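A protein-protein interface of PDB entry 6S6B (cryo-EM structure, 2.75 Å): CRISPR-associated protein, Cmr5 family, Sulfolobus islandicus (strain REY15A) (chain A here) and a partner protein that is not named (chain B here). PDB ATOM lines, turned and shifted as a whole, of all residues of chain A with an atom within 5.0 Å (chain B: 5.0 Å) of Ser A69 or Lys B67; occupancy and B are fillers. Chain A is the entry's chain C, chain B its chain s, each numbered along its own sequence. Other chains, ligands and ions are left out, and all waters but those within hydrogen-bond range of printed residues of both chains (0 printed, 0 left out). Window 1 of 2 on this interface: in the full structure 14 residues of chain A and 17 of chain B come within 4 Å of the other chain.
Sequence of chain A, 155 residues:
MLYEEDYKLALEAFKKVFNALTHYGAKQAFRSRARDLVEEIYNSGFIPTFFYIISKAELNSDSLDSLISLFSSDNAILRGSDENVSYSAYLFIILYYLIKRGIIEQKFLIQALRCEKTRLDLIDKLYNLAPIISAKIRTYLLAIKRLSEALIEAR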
ATOM      1  N   ASP A  65     -11.720   7.339  -3.025  1.00  0.00           N
ATOM      2  CA  ASP A  65     -11.352   8.650  -2.505  1.00  0.00           C
ATOM      3  C   ASP A  65     -11.075   9.634  -3.630  1.00  0.00           C
ATOM      4  O   ASP A  65     -11.521  10.786  -3.578  1.00  0.00           O
ATOM      5  CB  ASP A  65     -10.135   8.529  -1.595  1.00  0.00           C
ATOM      6  CG  ASP A  65      -9.698   9.858  -1.046  1.00  0.00           C
ATOM      7  OD1 ASP A  65     -10.412  10.401  -0.182  1.00  0.00           O
ATOM      8  OD2 ASP A  65      -8.642  10.363  -1.481  1.00  0.00           O
ATOM      9  N   SER A  66     -10.334   9.203  -4.651  1.00  0.00           N
ATOM     10  CA  SER A  66     -10.042  10.083  -5.774  1.00  0.00           C
ATOM     11  C   SER A  66     -11.310  10.449  -6.529  1.00  0.00           C
ATOM     12  O   SER A  66     -11.495  11.605  -6.925  1.00  0.00           O
ATOM     13  CB  SER A  66      -9.043   9.414  -6.712  1.00  0.00           C
ATOM     14  OG  SER A  66      -9.723   8.618  -7.663  1.00  0.00           O
ATOM     15  N   LEU A  67     -12.191   9.471  -6.742  1.00  0.00           N
ATOM     16  CA  LEU A  67     -13.444   9.728  -7.441  1.00  0.00           C
ATOM     17  C   LEU A  67     -14.251  10.815  -6.748  1.00  0.00           C
ATOM     18  O   LEU A  67     -14.841  11.676  -7.408  1.00  0.00           O
ATOM     19  CB  LEU A  67     -14.254   8.440  -7.538  1.00  0.00           C
ATOM     20  CG  LEU A  67     -15.388   8.395  -8.556  1.00  0.00           C
ATOM     21  CD1 LEU A  67     -15.462   7.022  -9.166  1.00  0.00           C
ATOM     22  CD2 LEU A  67     -16.707   8.748  -7.904  1.00  0.00           C
ATOM     23  N   ILE A  68     -14.291  10.793  -5.416  1.00  0.00           N
ATOM     24  CA  ILE A  68     -15.017  11.829  -4.692  1.00  0.00           C
ATOM     25  C   ILE A  68     -14.340  13.179  -4.874  1.00  0.00           C
ATOM     26  O   ILE A  68     -15.008  14.202  -5.058  1.00  0.00           O
ATOM     27  CB  ILE A  68     -15.144  11.456  -3.207  1.00  0.00           C
ATOM     28  CG1 ILE A  68     -15.939  10.162  -3.054  1.00  0.00           C
ATOM     29  CG2 ILE A  68     -15.822  12.572  -2.447  1.00  0.00           C
ATOM     30  CD1 ILE A  68     -15.733   9.479  -1.725  1.00  0.00           C
ATOM     31  N   SER A  69     -13.006  13.205  -4.833  1.00  0.00           N
ATOM     32  CA  SER A  69     -12.287  14.456  -5.040  1.00  0.00           C
ATOM     33  C   SER A  69     -12.602  15.061  -6.397  1.00  0.00           C
ATOM     34  O   SER A  69     -12.614  16.288  -6.543  1.00  0.00           O
ATOM     35  CB  SER A  69     -10.782  14.230  -4.906  1.00  0.00           C
ATOM     36  OG  SER A  69     -10.438  13.802  -3.603  1.00  0.00           O
ATOM     37  N   LEU A  70     -12.867  14.219  -7.395  1.00  0.00           N
ATOM     38  CA  LEU A  70     -13.079  14.712  -8.749  1.00  0.00           C
ATOM     39  C   LEU A  70     -14.346  15.551  -8.842  1.00  0.00           C
ATOM     40  O   LEU A  70     -14.442  16.434  -9.698  1.00  0.00           O
ATOM     41  CB  LEU A  70     -13.143  13.527  -9.712  1.00  0.00           C
ATOM     42  CG  LEU A  70     -12.802  13.697 -11.192  1.00  0.00           C
ATOM     43  CD1 LEU A  70     -12.434  12.344 -11.755  1.00  0.00           C
ATOM     44  CD2 LEU A  70     -13.913  14.307 -11.985  1.00  0.00           C
ATOM     45  N   PHE A  71     -15.317  15.300  -7.962  1.00  0.00           N
ATOM     46  CA  PHE A  71     -16.555  16.072  -7.976  1.00  0.00           C
ATOM     47  C   PHE A  71     -16.317  17.530  -7.626  1.00  0.00           C
ATOM     48  O   PHE A  71     -17.045  18.407  -8.104  1.00  0.00           O
ATOM     49  CB  PHE A  71     -17.562  15.463  -7.002  1.00  0.00           C
ATOM     50  CG  PHE A  71     -18.412  14.395  -7.611  1.00  0.00           C
ATOM     51  CD1 PHE A  71     -19.351  14.709  -8.577  1.00  0.00           C
ATOM     52  CD2 PHE A  71     -18.270  13.074  -7.224  1.00  0.00           C
ATOM     53  CE1 PHE A  71     -20.127  13.728  -9.144  1.00  0.00           C
ATOM     54  CE2 PHE A  71     -19.048  12.092  -7.787  1.00  0.00           C
ATOM     55  CZ  PHE A  71     -19.975  12.419  -8.749  1.00  0.00           C
ATOM     56  N   SER A  72     -15.314  17.811  -6.800  1.00  0.00           N
ATOM     57  CA  SER A  72     -15.068  19.154  -6.298  1.00  0.00           C
ATOM     58  C   SER A  72     -13.757  19.734  -6.808  1.00  0.00           C
ATOM     59  O   SER A  72     -13.748  20.812  -7.409  1.00  0.00           O
ATOM     60  CB  SER A  72     -15.081  19.131  -4.767  1.00  0.00           C
ATOM     61  OG  SER A  72     -14.016  18.340  -4.274  1.00  0.00           O
ATOM     62  N   SER A  73     -12.646  19.041  -6.594  1.00  0.00           N
ATOM     63  CA  SER A  73     -11.338  19.561  -6.961  1.00  0.00           C
ATOM     64  C   SER A  73     -11.139  19.436  -8.470  1.00  0.00           C
ATOM     65  O   SER A  73     -12.034  19.021  -9.211  1.00  0.00           O
ATOM     66  CB  SER A  73     -10.247  18.835  -6.180  1.00  0.00           C
ATOM     67  OG  SER A  73      -8.962  19.301  -6.546  1.00  0.00           O
ATOM     68  N   ALA A  76      -7.713  16.303  -8.919  1.00  0.00           N
ATOM     69  CA  ALA A  76      -8.010  14.897  -8.695  1.00  0.00           C
ATOM     70  C   ALA A  76      -7.663  14.081  -9.932  1.00  0.00           C
ATOM     71  O   ALA A  76      -7.958  14.478 -11.062  1.00  0.00           O
ATOM     72  CB  ALA A  76      -9.483  14.714  -8.338  1.00  0.00           C
ATOM     73  N   TYR B   7      -2.585  13.987  14.441  1.00  0.00           N
ATOM     74  CA  TYR B   7      -3.023  14.211  13.071  1.00  0.00           C
ATOM     75  C   TYR B   7      -2.894  15.692  12.755  1.00  0.00           C
ATOM     76  O   TYR B   7      -3.510  16.530  13.424  1.00  0.00           O
ATOM     77  CB  TYR B   7      -4.464  13.755  12.853  1.00  0.00           C
ATOM     78  CG  TYR B   7      -5.065  14.321  11.584  1.00  0.00           C
ATOM     79  CD1 TYR B   7      -4.807  13.732  10.352  1.00  0.00           C
ATOM     80  CD2 TYR B   7      -5.875  15.449  11.613  1.00  0.00           C
ATOM     81  CE1 TYR B   7      -5.343  14.245   9.189  1.00  0.00           C
ATOM     82  CE2 TYR B   7      -6.413  15.971  10.451  1.00  0.00           C
ATOM     83  CZ  TYR B   7      -6.143  15.363   9.242  1.00  0.00           C
ATOM     84  OH  TYR B   7      -6.679  15.871   8.081  1.00  0.00           O
ATOM     85  N   PHE B   9      -2.983  18.649   9.471  1.00  0.00           N
ATOM     86  CA  PHE B   9      -3.633  18.862   8.190  1.00  0.00           C
ATOM     87  C   PHE B   9      -2.721  19.648   7.259  1.00  0.00           C
ATOM     88  O   PHE B   9      -2.026  20.576   7.683  1.00  0.00           O
ATOM     89  CB  PHE B   9      -4.978  19.575   8.365  1.00  0.00           C
ATOM     90  CG  PHE B   9      -4.869  20.983   8.881  1.00  0.00           C
ATOM     91  CD1 PHE B   9      -5.037  21.253  10.226  1.00  0.00           C
ATOM     92  CD2 PHE B   9      -4.657  22.044   8.015  1.00  0.00           C
ATOM     93  CE1 PHE B   9      -4.954  22.545  10.704  1.00  0.00           C
ATOM     94  CE2 PHE B   9      -4.573  23.338   8.486  1.00  0.00           C
ATOM     95  CZ  PHE B   9      -4.725  23.589   9.831  1.00  0.00           C
ATOM     96  N   ILE B  10      -2.724  19.254   5.993  1.00  0.00           N
ATOM     97  CA  ILE B  10      -1.951  19.886   4.928  1.00  0.00           C
ATOM     98  C   ILE B  10      -2.502  21.243   4.479  1.00  0.00           C
ATOM     99  O   ILE B  10      -1.701  22.095   4.071  1.00  0.00           O
ATOM    100  CB  ILE B  10      -1.825  18.922   3.739  1.00  0.00           C
ATOM    101  CG1 ILE B  10      -1.258  17.592   4.232  1.00  0.00           C
ATOM    102  CG2 ILE B  10      -0.930  19.498   2.658  1.00  0.00           C
ATOM    103  CD1 ILE B  10       0.089  17.710   4.909  1.00  0.00           C
ATOM    104  N   PRO B  11      -3.853  21.509   4.526  1.00  0.00           N
ATOM    105  CA  PRO B  11      -4.402  22.745   3.936  1.00  0.00           C
ATOM    106  C   PRO B  11      -3.583  24.017   4.095  1.00  0.00           C
ATOM    107  O   PRO B  11      -2.910  24.230   5.108  1.00  0.00           O
ATOM    108  CB  PRO B  11      -5.741  22.883   4.662  1.00  0.00           C
ATOM    109  CG  PRO B  11      -6.181  21.489   4.849  1.00  0.00           C
ATOM    110  CD  PRO B  11      -4.960  20.598   4.871  1.00  0.00           C
ATOM    111  N   VAL B  41      -2.290   7.882   4.102  1.00  0.00           N
ATOM    112  CA  VAL B  41      -2.986   9.133   4.373  1.00  0.00           C
ATOM    113  C   VAL B  41      -4.299   8.826   5.073  1.00  0.00           C
ATOM    114  O   VAL B  41      -4.954   7.816   4.786  1.00  0.00           O
ATOM    115  CB  VAL B  41      -3.225   9.910   3.068  1.00  0.00           C
ATOM    116  CG1 VAL B  41      -3.679  11.328   3.361  1.00  0.00           C
ATOM    117  CG2 VAL B  41      -1.989   9.896   2.199  1.00  0.00           C
ATOM    118  N   LEU B  42      -4.694   9.693   5.998  1.00  0.00           N
ATOM    119  CA  LEU B  42      -5.899   9.485   6.789  1.00  0.00           C
ATOM    120  C   LEU B  42      -6.841  10.659   6.577  1.00  0.00           C
ATOM    121  O   LEU B  42      -6.510  11.798   6.922  1.00  0.00           O
ATOM    122  CB  LEU B  42      -5.559   9.314   8.270  1.00  0.00           C
ATOM    123  CG  LEU B  42      -6.743   9.187   9.226  1.00  0.00           C
ATOM    124  CD1 LEU B  42      -6.512   8.049  10.196  1.00  0.00           C
ATOM    125  CD2 LEU B  42      -6.939  10.481   9.982  1.00  0.00           C
ATOM    126  N   VAL B  43      -8.010  10.376   6.013  1.00  0.00           N
ATOM    127  CA  VAL B  43      -9.017  11.381   5.697  1.00  0.00           C
ATOM    128  C   VAL B  43     -10.079  11.397   6.789  1.00  0.00           C
ATOM    129  O   VAL B  43     -10.526  10.342   7.258  1.00  0.00           O
ATOM    130  CB  VAL B  43      -9.632  11.114   4.307  1.00  0.00           C
ATOM    131  CG1 VAL B  43     -10.371   9.791   4.287  1.00  0.00           C
ATOM    132  CG2 VAL B  43     -10.576  12.231   3.905  1.00  0.00           C
ATOM    133  N   TYR B  65     -14.677  17.290   3.666  1.00  0.00           N
ATOM    134  CA  TYR B  65     -13.694  16.413   4.285  1.00  0.00           C
ATOM    135  C   TYR B  65     -12.367  17.150   4.375  1.00  0.00           C
ATOM    136  O   TYR B  65     -12.223  18.273   3.887  1.00  0.00           O
ATOM    137  CB  TYR B  65     -13.552  15.111   3.495  1.00  0.00           C
ATOM    138  CG  TYR B  65     -13.319  15.315   2.014  1.00  0.00           C
ATOM    139  CD1 TYR B  65     -14.386  15.457   1.137  1.00  0.00           C
ATOM    140  CD2 TYR B  65     -12.034  15.360   1.492  1.00  0.00           C
ATOM    141  CE1 TYR B  65     -14.179  15.643  -0.216  1.00  0.00           C
ATOM    142  CE2 TYR B  65     -11.818  15.545   0.141  1.00  0.00           C
ATOM    143  CZ  TYR B  65     -12.893  15.684  -0.708  1.00  0.00           C
ATOM    144  OH  TYR B  65     -12.685  15.869  -2.055  1.00  0.00           O
ATOM    145  N   VAL B  66     -11.391  16.498   5.011  1.00  0.00           N
ATOM    146  CA  VAL B  66     -10.044  17.029   5.171  1.00  0.00           C
ATOM    147  C   VAL B  66      -9.056  15.885   4.997  1.00  0.00           C
ATOM    148  O   VAL B  66      -9.381  14.717   5.212  1.00  0.00           O
ATOM    149  CB  VAL B  66      -9.831  17.689   6.548  1.00  0.00           C
ATOM    150  CG1 VAL B  66     -10.819  18.816   6.759  1.00  0.00           C
ATOM    151  CG2 VAL B  66      -9.950  16.652   7.643  1.00  0.00           C
ATOM    152  N   LYS B  67      -7.830  16.231   4.618  1.00  0.00           N
ATOM    153  CA  LYS B  67      -6.772  15.241   4.475  1.00  0.00           C
ATOM    154  C   LYS B  67      -5.468  15.807   5.015  1.00  0.00           C
ATOM    155  O   LYS B  67      -5.162  16.985   4.807  1.00  0.00           O
ATOM    156  CB  LYS B  67      -6.594  14.812   3.012  1.00  0.00           C
ATOM    157  CG  LYS B  67      -7.751  13.993   2.459  1.00  0.00           C
ATOM    158  CD  LYS B  67      -7.757  13.985   0.942  1.00  0.00           C
ATOM    159  CE  LYS B  67      -9.020  13.339   0.403  1.00  0.00           C
ATOM    160  NZ  LYS B  67      -8.945  13.112  -1.066  1.00  0.00           N
ATOM    161  N   GLY B  68      -4.708  14.970   5.698  1.00  0.00           N
ATOM    162  CA  GLY B  68      -3.450  15.389   6.282  1.00  0.00           C
ATOM    163  C   GLY B  68      -2.543  14.221   6.601  1.00  0.00           C
ATOM    164  O   GLY B  68      -2.558  13.196   5.915  1.00  0.00           O
ATOM    165  N   ILE B  69      -1.747  14.379   7.658  1.00  0.00           N
ATOM    166  CA  ILE B  69      -0.749  13.396   8.062  1.00  0.00           C
ATOM    167  C   ILE B  69      -1.051  12.954   9.487  1.00  0.00           C
ATOM    168  O   ILE B  69      -1.490  13.758  10.315  1.00  0.00           O
ATOM    169  CB  ILE B  69       0.680  13.970   7.958  1.00  0.00           C
ATOM    170  CG1 ILE B  69       0.944  14.499   6.550  1.00  0.00           C
ATOM    171  CG2 ILE B  69       1.711  12.912   8.303  1.00  0.00           C
ATOM    172  CD1 ILE B  69       0.853  13.446   5.473  1.00  0.00           C
ATOM    173  N   ILE B  96      -6.313   6.193   3.213  1.00  0.00           N
ATOM    174  CA  ILE B  96      -6.244   6.167   1.762  1.00  0.00           C
ATOM    175  C   ILE B  96      -4.782   6.003   1.374  1.00  0.00           C
ATOM    176  O   ILE B  96      -3.874   6.280   2.160  1.00  0.00           O
ATOM    177  CB  ILE B  96      -6.851   7.432   1.115  1.00  0.00           C
ATOM    178  CG1 ILE B  96      -5.993   8.651   1.430  1.00  0.00           C
ATOM    179  CG2 ILE B  96      -8.273   7.647   1.602  1.00  0.00           C
ATOM    180  CD1 ILE B  96      -6.571   9.960   0.952  1.00  0.00           C
ATOM    181  N   LEU B 166      -3.896  14.554  -3.732  1.00  0.00           N
ATOM    182  CA  LEU B 166      -4.675  14.068  -2.597  1.00  0.00           C
ATOM    183  C   LEU B 166      -5.200  15.212  -1.742  1.00  0.00           C
ATOM    184  O   LEU B 166      -6.415  15.365  -1.569  1.00  0.00           O
ATOM    185  CB  LEU B 166      -3.840  13.110  -1.746  1.00  0.00           C
ATOM    186  CG  LEU B 166      -3.656  11.694  -2.288  1.00  0.00           C
ATOM    187  CD1 LEU B 166      -2.403  11.588  -3.126  1.00  0.00           C
ATOM    188  CD2 LEU B 166      -3.610  10.717  -1.131  1.00  0.00           C
ATOM    189  N   PHE B 167      -4.306  16.042  -1.214  1.00  0.00           N
ATOM    190  CA  PHE B 167      -4.681  16.886  -0.087  1.00  0.00           C
ATOM    191  C   PHE B 167      -5.625  18.012  -0.483  1.00  0.00           C
ATOM    192  O   PHE B 167      -5.291  19.192  -0.350  1.00  0.00           O
ATOM    193  CB  PHE B 167      -3.431  17.450   0.583  1.00  0.00           C
ATOM    194  CG  PHE B 167      -2.599  16.408   1.253  1.00  0.00           C
ATOM    195  CD1 PHE B 167      -3.165  15.553   2.177  1.00  0.00           C
ATOM    196  CD2 PHE B 167      -1.257  16.273   0.956  1.00  0.00           C
ATOM    197  CE1 PHE B 167      -2.409  14.585   2.796  1.00  0.00           C
ATOM    198  CE2 PHE B 167      -0.495  15.307   1.572  1.00  0.00           C
ATOM    199  CZ  PHE B 167      -1.072  14.461   2.494  1.00  0.00           C
ATOM    200  N   SER B 168      -6.814  17.651  -0.947  1.00  0.00           N
ATOM    201  CA  SER B 168      -7.907  18.598  -1.024  1.00  0.00           C
ATOM    202  C   SER B 168      -8.565  18.723   0.345  1.00  0.00           C
ATOM    203  O   SER B 168      -8.286  17.951   1.268  1.00  0.00           O
ATOM    204  CB  SER B 168      -8.922  18.156  -2.074  1.00  0.00           C
ATOM    205  OG  SER B 168      -9.212  16.776  -1.941  1.00  0.00           O
ATOM    206  N   TYR B 169      -9.457  19.698   0.476  1.00  0.00           N
ATOM    207  CA  TYR B 169     -10.137  19.935   1.743  1.00  0.00           C
ATOM    208  C   TYR B 169     -11.232  20.961   1.509  1.00  0.00           C
ATOM    209  O   TYR B 169     -11.332  21.561   0.437  1.00  0.00           O
ATOM    210  CB  TYR B 169      -9.172  20.417   2.827  1.00  0.00           C
ATOM    211  CG  TYR B 169      -8.556  21.758   2.525  1.00  0.00           C
ATOM    212  CD1 TYR B 169      -7.515  21.878   1.616  1.00  0.00           C
ATOM    213  CD2 TYR B 169      -9.013  22.902   3.152  1.00  0.00           C
ATOM    214  CE1 TYR B 169      -6.955  23.100   1.339  1.00  0.00           C
ATOM    215  CE2 TYR B 169      -8.457  24.125   2.883  1.00  0.00           C
ATOM    216  CZ  TYR B 169      -7.432  24.220   1.977  1.00  0.00           C
ATOM    217  OH  TYR B 169      -6.881  25.451   1.716  1.00  0.00           O
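OH of Tyr B65 lies close to OG of Ser A69, at 3.4 Å.
The side-chain carboxylate (OD2) of Asp A65 lies within salt-bridge range of the side-chain amino group (NZ) of Lys B67 (2.8 Å).
The side-chain hydroxyl (OG) of Ser A69 is in hydrogen-bond range of the side-chain amino group (NZ) of Lys B67, at 3.0 Å.
The side-chain hydroxyl (OG) of Ser A72 sits at hydrogen-bond distance from the backbone carbonyl oxygen (O) of Ser A69 (3.4 Å).
O of Val B41 sits at hydrogen-bond distance from N of Ile B96, 2.6 Å away.
The backbone carbonyl oxygen (O) of Asp A65 lies within hydrogen-bond range of the side-chain hydroxyl (OG) of Ser A69 (3.2 Å).
The backbone carbonyl oxygen of Leu B166 is in hydrogen-bond range of the side-chain hydroxyl of Ser B168 (3.2 Å).
NZ of Lys B67 lies close to O of Leu B166.
Among the printed residues, merely in contact across the chains: Asp A65 with Ile B96, Ser A72 with Tyr B65 and Ser A69 with Ser B168.
Printed residues of chain B within 4 Å of Asp A65: Lys B67 and Ile B96.
Ser A69 touches three residues of chain B.
Printed residues of chain B within 4 Å of Ser A72: Tyr B65 (3.6 Å).
Printed residues of chain A within 4 Å of Tyr B65: Ser A69 (3.3 Å) and Ser A72 (3.6 Å).
Lys B67 touches two residues of chain A.
Printed residues of chain A within 4 Å of Ser B168: Ser A69 (3.6 Å).
The nearest residue of chain B that does not touch Ser A69 is Leu B166 (4.8 Å).
The nearest printed residue of chain A that does not touch Lys B67 is Ser A66 (5.5 Å).
Of the 17 printed residues of chain B, 4 touch a printed residue of chain A.
Along chain B the printed residues that touch a printed residue of chain A span positions 65 to 168.
Among the printed residues, 6 pairs touch across the chains.
Among the printed residues, Asp or Glu carboxylates within 4 Å of a Lys or Arg side-chain nitrogen of the other chain: Asp A65 with Lys B67.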
